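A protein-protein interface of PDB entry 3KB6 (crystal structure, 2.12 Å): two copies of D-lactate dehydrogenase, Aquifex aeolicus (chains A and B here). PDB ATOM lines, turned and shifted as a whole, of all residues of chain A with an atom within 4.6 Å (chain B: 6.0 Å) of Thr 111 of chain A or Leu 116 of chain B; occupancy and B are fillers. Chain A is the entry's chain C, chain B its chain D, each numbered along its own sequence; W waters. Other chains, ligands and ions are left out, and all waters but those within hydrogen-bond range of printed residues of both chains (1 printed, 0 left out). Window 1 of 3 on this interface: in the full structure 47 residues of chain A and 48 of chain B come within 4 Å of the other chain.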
ATOM      1  N   HIS A 104       3.133  27.343  35.972  1.00  0.00           N
ATOM      2  CA  HIS A 104       3.921  28.059  34.969  1.00  0.00           C
ATOM      3  C   HIS A 104       5.125  28.769  35.588  1.00  0.00           C
ATOM      4  O   HIS A 104       6.235  28.692  35.072  1.00  0.00           O
ATOM      5  CB  HIS A 104       3.057  29.046  34.221  1.00  0.00           C
ATOM      6  CG  HIS A 104       3.683  29.512  32.951  1.00  0.00           C
ATOM      7  ND1 HIS A 104       3.732  28.726  31.826  1.00  0.00           N
ATOM      8  CD2 HIS A 104       4.328  30.666  32.644  1.00  0.00           C
ATOM      9  CE1 HIS A 104       4.343  29.397  30.861  1.00  0.00           C
ATOM     10  NE2 HIS A 104       4.717  30.576  31.330  1.00  0.00           N
ATOM     11  N   ALA A 107       7.712  26.271  36.235  1.00  0.00           N
ATOM     12  CA  ALA A 107       8.269  25.803  34.953  1.00  0.00           C
ATOM     13  C   ALA A 107       9.386  26.751  34.479  1.00  0.00           C
ATOM     14  O   ALA A 107      10.508  26.294  34.056  1.00  0.00           O
ATOM     15  CB  ALA A 107       7.170  25.683  33.904  1.00  0.00           C
ATOM     16  N   MET A 108       9.146  28.062  34.644  1.00  0.00           N
ATOM     17  CA  MET A 108      10.166  29.059  34.324  1.00  0.00           C
ATOM     18  C   MET A 108      11.354  29.043  35.256  1.00  0.00           C
ATOM     19  O   MET A 108      12.517  29.056  34.799  1.00  0.00           O
ATOM     20  CB  MET A 108       9.572  30.468  34.281  1.00  0.00           C
ATOM     21  CG  MET A 108       8.536  30.678  33.190  1.00  0.00           C
ATOM     22  SD  MET A 108       7.974  32.624  33.139  1.00  0.00           S
ATOM     23  CE  MET A 108       7.478  32.666  31.276  1.00  0.00           C
ATOM     24  N   ILE A 109      11.110  29.023  36.559  1.00  0.00           N
ATOM     25  CA  ILE A 109      12.216  28.890  37.503  1.00  0.00           C
ATOM     26  C   ILE A 109      13.097  27.665  37.152  1.00  0.00           C
ATOM     27  O   ILE A 109      14.290  27.762  37.021  1.00  0.00           O
ATOM     28  CB  ILE A 109      11.692  28.759  38.993  1.00  0.00           C
ATOM     29  CG1 ILE A 109      10.996  30.054  39.450  1.00  0.00           C
ATOM     30  CG2 ILE A 109      12.820  28.504  39.946  1.00  0.00           C
ATOM     31  CD1 ILE A 109      10.312  29.961  40.818  1.00  0.00           C
ATOM     32  N   LEU A 110      12.495  26.496  37.040  1.00  0.00           N
ATOM     33  CA  LEU A 110      13.267  25.292  36.734  1.00  0.00           C
ATOM     34  C   LEU A 110      14.004  25.384  35.386  1.00  0.00           C
ATOM     35  O   LEU A 110      15.156  24.945  35.263  1.00  0.00           O
ATOM     36  CB  LEU A 110      12.363  24.053  36.801  1.00  0.00           C
ATOM     37  CG  LEU A 110      12.104  23.579  38.245  1.00  0.00           C
ATOM     38  CD1 LEU A 110      11.047  22.559  38.259  1.00  0.00           C
ATOM     39  CD2 LEU A 110      13.399  23.061  38.872  1.00  0.00           C
ATOM     40  N   THR A 111      13.364  25.997  34.407  1.00  0.00           N
ATOM     41  CA  THR A 111      13.991  26.199  33.089  1.00  0.00           C
ATOM     42  C   THR A 111      15.256  26.997  33.227  1.00  0.00           C
ATOM     43  O   THR A 111      16.284  26.662  32.638  1.00  0.00           O
ATOM     44  CB  THR A 111      13.041  26.933  32.130  1.00  0.00           C
ATOM     45  OG1 THR A 111      11.915  26.091  31.885  1.00  0.00           O
ATOM     46  CG2 THR A 111      13.732  27.267  30.794  1.00  0.00           C
ATOM     47  N   LEU A 112      15.181  28.051  34.026  1.00  0.00           N
ATOM     48  CA  LEU A 112      16.283  28.950  34.175  1.00  0.00           C
ATOM     49  C   LEU A 112      17.408  28.360  35.010  1.00  0.00           C
ATOM     50  O   LEU A 112      18.583  28.415  34.598  1.00  0.00           O
ATOM     51  CB  LEU A 112      15.808  30.274  34.740  1.00  0.00           C
ATOM     52  CG  LEU A 112      14.874  31.076  33.809  1.00  0.00           C
ATOM     53  CD1 LEU A 112      14.132  32.182  34.600  1.00  0.00           C
ATOM     54  CD2 LEU A 112      15.673  31.610  32.549  1.00  0.00           C
ATOM     55  N   VAL A 113      17.073  27.751  36.151  1.00  0.00           N
ATOM     56  CA  VAL A 113      18.102  27.256  37.074  1.00  0.00           C
ATOM     57  C   VAL A 113      18.825  26.011  36.493  1.00  0.00           C
ATOM     58  O   VAL A 113      20.018  25.768  36.772  1.00  0.00           O
ATOM     59  CB  VAL A 113      17.457  26.913  38.486  1.00  0.00           C
ATOM     60  CG1 VAL A 113      18.325  26.013  39.242  1.00  0.00           C
ATOM     61  CG2 VAL A 113      17.196  28.218  39.315  1.00  0.00           C
ATOM     62  N   LYS A 114      18.100  25.213  35.724  1.00  0.00           N
ATOM     63  CA  LYS A 114      18.714  24.055  35.060  1.00  0.00           C
ATOM     64  C   LYS A 114      19.314  24.379  33.663  1.00  0.00           C
ATOM     65  O   LYS A 114      19.836  23.493  32.991  1.00  0.00           O
ATOM     66  CB  LYS A 114      17.726  22.888  34.981  1.00  0.00           C
ATOM     67  CG  LYS A 114      17.165  22.402  36.366  1.00  0.00           C
ATOM     68  CD  LYS A 114      18.273  22.068  37.372  1.00  0.00           C
ATOM     69  CE  LYS A 114      17.703  21.661  38.797  1.00  0.00           C
ATOM     70  NZ  LYS A 114      18.787  21.410  39.855  1.00  0.00           N
ATOM     71  N   ARG A 115      19.230  25.640  33.245  1.00  0.00           N
ATOM     72  CA  ARG A 115      19.896  26.127  32.034  1.00  0.00           C
ATOM     73  C   ARG A 115      19.489  25.344  30.806  1.00  0.00           C
ATOM     74  O   ARG A 115      20.311  25.018  29.966  1.00  0.00           O
ATOM     75  CB  ARG A 115      21.415  26.085  32.245  1.00  0.00           C
ATOM     76  CG  ARG A 115      21.782  26.789  33.543  1.00  0.00           C
ATOM     77  CD  ARG A 115      23.200  26.896  33.792  1.00  0.00           C
ATOM     78  NE  ARG A 115      23.753  28.025  33.072  1.00  0.00           N
ATOM     79  CZ  ARG A 115      25.002  28.470  33.209  1.00  0.00           C
ATOM     80  NH1 ARG A 115      25.847  27.877  34.059  1.00  0.00           N
ATOM     81  NH2 ARG A 115      25.406  29.515  32.477  1.00  0.00           N
ATOM     82  N   LEU A 116      18.203  25.051  30.700  1.00  0.00           N
ATOM     83  CA  LEU A 116      17.705  24.181  29.650  1.00  0.00           C
ATOM     84  C   LEU A 116      17.793  24.804  28.245  1.00  0.00           C
ATOM     85  O   LEU A 116      17.987  24.079  27.255  1.00  0.00           O
ATOM     86  CB  LEU A 116      16.271  23.784  29.942  1.00  0.00           C
ATOM     87  CG  LEU A 116      15.970  22.974  31.224  1.00  0.00           C
ATOM     88  CD1 LEU A 116      14.464  22.526  31.172  1.00  0.00           C
ATOM     89  CD2 LEU A 116      16.870  21.738  31.309  1.00  0.00           C
ATOM     90  N   ILE A 290      13.532  33.562  29.428  1.00  0.00           N
ATOM     91  CA  ILE A 290      12.370  32.964  28.832  1.00  0.00           C
ATOM     92  C   ILE A 290      11.272  33.983  28.850  1.00  0.00           C
ATOM     93  O   ILE A 290      10.904  34.494  29.924  1.00  0.00           O
ATOM     94  CB  ILE A 290      11.930  31.566  29.489  1.00  0.00           C
ATOM     95  CG1 ILE A 290      10.582  31.104  28.898  1.00  0.00           C
ATOM     96  CG2 ILE A 290      11.858  31.623  30.989  1.00  0.00           C
ATOM     97  CD1 ILE A 290      10.120  29.698  29.358  1.00  0.00           C
ATOM     98  N   ALA B 107      11.878  19.583  36.021  1.00  0.00           N
ATOM     99  CA  ALA B 107      12.090  20.605  35.000  1.00  0.00           C
ATOM    100  C   ALA B 107      11.641  20.083  33.636  1.00  0.00           C
ATOM    101  O   ALA B 107      10.929  20.791  32.910  1.00  0.00           O
ATOM    102  CB  ALA B 107      13.564  21.099  34.974  1.00  0.00           C
ATOM    103  N   LEU B 110       7.657  19.697  33.574  1.00  0.00           N
ATOM    104  CA  LEU B 110       7.050  21.051  33.433  1.00  0.00           C
ATOM    105  C   LEU B 110       7.273  21.664  32.041  1.00  0.00           C
ATOM    106  O   LEU B 110       6.324  22.182  31.428  1.00  0.00           O
ATOM    107  CB  LEU B 110       7.544  21.972  34.542  1.00  0.00           C
ATOM    108  CG  LEU B 110       6.825  21.743  35.895  1.00  0.00           C
ATOM    109  CD1 LEU B 110       7.558  22.402  37.035  1.00  0.00           C
ATOM    110  CD2 LEU B 110       5.399  22.252  35.823  1.00  0.00           C
ATOM    111  N   THR B 111       8.493  21.525  31.523  1.00  0.00           N
ATOM    112  CA  THR B 111       8.793  21.944  30.158  1.00  0.00           C
ATOM    113  C   THR B 111       7.792  21.383  29.175  1.00  0.00           C
ATOM    114  O   THR B 111       7.269  22.112  28.334  1.00  0.00           O
ATOM    115  CB  THR B 111      10.185  21.530  29.731  1.00  0.00           C
ATOM    116  OG1 THR B 111      11.153  22.236  30.505  1.00  0.00           O
ATOM    117  CG2 THR B 111      10.450  21.827  28.250  1.00  0.00           C
ATOM    118  N   LEU B 112       7.507  20.090  29.281  1.00  0.00           N
ATOM    119  CA  LEU B 112       6.697  19.407  28.291  1.00  0.00           C
ATOM    120  C   LEU B 112       5.240  19.719  28.458  1.00  0.00           C
ATOM    121  O   LEU B 112       4.518  19.970  27.464  1.00  0.00           O
ATOM    122  CB  LEU B 112       6.919  17.884  28.333  1.00  0.00           C
ATOM    123  CG  LEU B 112       8.331  17.403  27.990  1.00  0.00           C
ATOM    124  CD1 LEU B 112       8.606  15.906  28.437  1.00  0.00           C
ATOM    125  CD2 LEU B 112       8.542  17.575  26.440  1.00  0.00           C
ATOM    126  N   VAL B 113       4.786  19.723  29.717  1.00  0.00           N
ATOM    127  CA  VAL B 113       3.353  19.885  29.978  1.00  0.00           C
ATOM    128  C   VAL B 113       2.964  21.341  29.709  1.00  0.00           C
ATOM    129  O   VAL B 113       1.861  21.621  29.251  1.00  0.00           O
ATOM    130  CB  VAL B 113       3.006  19.492  31.440  1.00  0.00           C
ATOM    131  CG1 VAL B 113       1.605  19.930  31.788  1.00  0.00           C
ATOM    132  CG2 VAL B 113       3.166  17.969  31.613  1.00  0.00           C
ATOM    133  N   LYS B 114       3.875  22.263  29.985  1.00  0.00           N
ATOM    134  CA  LYS B 114       3.640  23.694  29.681  1.00  0.00           C
ATOM    135  C   LYS B 114       3.990  24.104  28.225  1.00  0.00           C
ATOM    136  O   LYS B 114       3.817  25.276  27.827  1.00  0.00           O
ATOM    137  CB  LYS B 114       4.363  24.575  30.715  1.00  0.00           C
ATOM    138  CG  LYS B 114       3.838  24.402  32.188  1.00  0.00           C
ATOM    139  CD  LYS B 114       2.326  24.146  32.268  1.00  0.00           C
ATOM    140  CE  LYS B 114       1.791  23.845  33.758  1.00  0.00           C
ATOM    141  NZ  LYS B 114       0.206  23.893  33.955  1.00  0.00           N
ATOM    142  N   ARG B 115       4.462  23.128  27.445  1.00  0.00           N
ATOM    143  CA  ARG B 115       4.760  23.295  26.046  1.00  0.00           C
ATOM    144  C   ARG B 115       5.698  24.439  25.775  1.00  0.00           C
ATOM    145  O   ARG B 115       5.508  25.179  24.823  1.00  0.00           O
ATOM    146  CB  ARG B 115       3.452  23.436  25.296  1.00  0.00           C
ATOM    147  CG  ARG B 115       2.562  22.278  25.693  1.00  0.00           C
ATOM    148  CD  ARG B 115       1.283  22.260  25.005  1.00  0.00           C
ATOM    149  NE  ARG B 115       1.442  21.646  23.719  1.00  0.00           N
ATOM    150  CZ  ARG B 115       0.447  21.445  22.859  1.00  0.00           C
ATOM    151  NH1 ARG B 115      -0.826  21.803  23.148  1.00  0.00           N
ATOM    152  NH2 ARG B 115       0.741  20.885  21.695  1.00  0.00           N
ATOM    153  N   LEU B 116       6.737  24.557  26.603  1.00  0.00           N
ATOM    154  CA  LEU B 116       7.640  25.697  26.541  1.00  0.00           C
ATOM    155  C   LEU B 116       8.452  25.725  25.220  1.00  0.00           C
ATOM    156  O   LEU B 116       8.755  26.800  24.687  1.00  0.00           O
ATOM    157  CB  LEU B 116       8.594  25.738  27.736  1.00  0.00           C
ATOM    158  CG  LEU B 116       7.970  25.835  29.140  1.00  0.00           C
ATOM    159  CD1 LEU B 116       9.038  25.982  30.243  1.00  0.00           C
ATOM    160  CD2 LEU B 116       6.985  27.027  29.199  1.00  0.00           C
ATOM    161  N   LYS B 117       8.786  24.546  24.694  1.00  0.00           N
ATOM    162  CA  LYS B 117       9.623  24.484  23.492  1.00  0.00           C
ATOM    163  C   LYS B 117       8.795  24.973  22.299  1.00  0.00           C
ATOM    164  O   LYS B 117       9.275  25.746  21.482  1.00  0.00           O
ATOM    165  CB  LYS B 117      10.181  23.046  23.325  1.00  0.00           C
ATOM    166  CG  LYS B 117      11.262  22.873  22.279  1.00  0.00           C
ATOM    167  CD  LYS B 117      11.867  21.484  22.372  1.00  0.00           C
ATOM    168  CE  LYS B 117      12.845  21.309  21.245  1.00  0.00           C
ATOM    169  NZ  LYS B 117      13.606  20.066  21.352  1.00  0.00           N
ATOM    170  N   ARG B 118       7.526  24.585  22.217  1.00  0.00           N
ATOM    171  CA  ARG B 118       6.687  25.093  21.147  1.00  0.00           C
ATOM    172  C   ARG B 118       6.425  26.602  21.244  1.00  0.00           C
ATOM    173  O   ARG B 118       6.437  27.306  20.242  1.00  0.00           O
ATOM    174  CB  ARG B 118       5.379  24.371  21.108  1.00  0.00           C
ATOM    175  CG  ARG B 118       4.475  24.890  20.063  1.00  0.00           C
ATOM    176  CD  ARG B 118       3.240  24.020  19.952  1.00  0.00           C
ATOM    177  NE  ARG B 118       3.496  22.825  19.173  1.00  0.00           N
ATOM    178  CZ  ARG B 118       2.553  22.064  18.619  1.00  0.00           C
ATOM    179  NH1 ARG B 118       1.268  22.360  18.762  1.00  0.00           N
ATOM    180  NH2 ARG B 118       2.899  20.986  17.919  1.00  0.00           N
ATOM    181  N   ILE B 119       6.204  27.093  22.461  1.00  0.00           N
ATOM    182  CA  ILE B 119       5.979  28.497  22.685  1.00  0.00           C
ATOM    183  C   ILE B 119       7.210  29.319  22.279  1.00  0.00           C
ATOM    184  O   ILE B 119       7.081  30.323  21.594  1.00  0.00           O
ATOM    185  CB  ILE B 119       5.564  28.759  24.156  1.00  0.00           C
ATOM    186  CG1 ILE B 119       4.133  28.225  24.398  1.00  0.00           C
ATOM    187  CG2 ILE B 119       5.691  30.233  24.471  1.00  0.00           C
ATOM    188  CD1 ILE B 119       3.786  27.954  25.897  1.00  0.00           C
ATOM    189  N   GLU B 120       8.388  28.868  22.686  1.00  0.00           N
ATOM    190  CA  GLU B 120       9.649  29.455  22.282  1.00  0.00           C
ATOM    191  C   GLU B 120       9.797  29.550  20.716  1.00  0.00           C
ATOM    192  O   GLU B 120      10.205  30.579  20.197  1.00  0.00           O
ATOM    193  CB  GLU B 120      10.780  28.644  22.915  1.00  0.00           C
ATOM    194  CG  GLU B 120      12.214  29.149  22.682  1.00  0.00           C
ATOM    195  CD  GLU B 120      13.305  28.066  22.941  1.00  0.00           C
ATOM    196  OE1 GLU B 120      12.991  26.897  23.270  1.00  0.00           O
ATOM    197  OE2 GLU B 120      14.499  28.402  22.793  1.00  0.00           O
ATOM    198  N   ASP B 121       9.425  28.504  19.982  1.00  0.00           N
ATOM    199  CA  ASP B 121       9.517  28.518  18.520  1.00  0.00           C
ATOM    200  C   ASP B 121       8.611  29.611  17.986  1.00  0.00           C
ATOM    201  O   ASP B 121       8.967  30.293  17.022  1.00  0.00           O
ATOM    202  CB  ASP B 121       9.028  27.203  17.886  1.00  0.00           C
ATOM    203  CG  ASP B 121       9.931  26.000  18.166  1.00  0.00           C
ATOM    204  OD1 ASP B 121      11.152  26.165  18.377  1.00  0.00           O
ATOM    205  OD2 ASP B 121       9.391  24.857  18.150  1.00  0.00           O
HETATM  206  O   HOH W   1      12.080  24.533  29.589  1.00  0.00           O
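Ala 107 of chain A touches Leu 110 of chain B, and with the chains exchanged Leu 110 of chain A touches Ala 107 of chain B.
Ala 107 of chain A touches Lys 114 of chain B, but with the chains exchanged Lys 114 of chain A does not touch Ala 107 of chain B (4.1 Å).
Leu 110 of chain B touches its own counterpart, Leu 110 of chain A.
Thr 111 of chain A touches Leu 116 of chain B, and with the chains exchanged Leu 116 of chain A touches Thr 111 of chain B.
Of the 8 pairs that touch across the chains among the printed residues, 5 have their exchanged pair printed and touching as well.
Thr 111 of chain A touches just one residue of chain B: Leu 116 (3.3 Å).
Printed residues of chain A within 4 Å of Leu 116 of chain B: His 104, Thr 111 and Ile 290.
Printed residues of chain A within 4 Å of Lys 114 of chain B: Ala 107.
Of the printed residues of chain B, Leu 116 of chain A touches Thr 111.
Printed residues of chain A within 4 Å of Ala 107 of chain B: Leu 110.
Printed residues of chain B within 4 Å of Leu 110 of chain A: Ala 107 and Leu 110.
Of the printed residues of chain B, Ile 290 of chain A touches Leu 116.
The nearest printed residue of chain A that does not touch Ala 107 of chain B is Lys 114 of chain A (4.1 Å).
Among the printed residues, pairs that only touch across the chains: His 104 of chain A with Leu 116 of chain B (3.9 Å), Ala 107 of chain A with Leu 110 of chain B (3.8 Å), Ala 107 of chain A with Lys 114 of chain B (3.96 Å), Leu 110 of chain A with Ala 107 of chain B (3.7 Å), Leu 110 of chain A with Leu 110 of chain B (3.7 Å), Thr 111 of chain A with Leu 116 of chain B (3.3 Å), Leu 116 of chain A with Thr 111 of chain B (3.4 Å) and Ile 290 of chain A with Leu 116 of chain B (3.97 Å).
The backbone carbonyl oxygen of Ala 107 of chain A lies within hydrogen-bond range of the side-chain hydroxyl of Thr 111 of chain A.
N of Leu 116 of chain B sits at hydrogen-bond distance from O of Thr 111 of chain B, 3.0 Å away.
O of Thr 111 of chain A lies within hydrogen-bond range of N of Leu 116 of chain A (3.2 Å).
OG1 of Thr 111 of chain B sits at hydrogen-bond distance from O of Ala 107 of chain B, 2.8 Å away.
Printed residues of chain A that touch a printed residue of chain B: His 104, Ala 107, Leu 110, Thr 111, Leu 116 and Ile 290.
Hydrophobic or aromatic side chains of chain A within 4 Å of the printed part of chain B: His 104, Ala 107, Leu 110, Leu 116 and Ile 290.
Of the 13 printed residues of chain B, 5 touch a printed residue of chain A.
Among the printed residues, no Asp or Glu carboxylate lies within 4 Å of a Lys or Arg side-chain nitrogen of the other chain.
Water W1 bridges OG1 of Thr 111 of chain B (2.6 Å) and OG1 of Thr 111 of chain A (2.8 Å).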
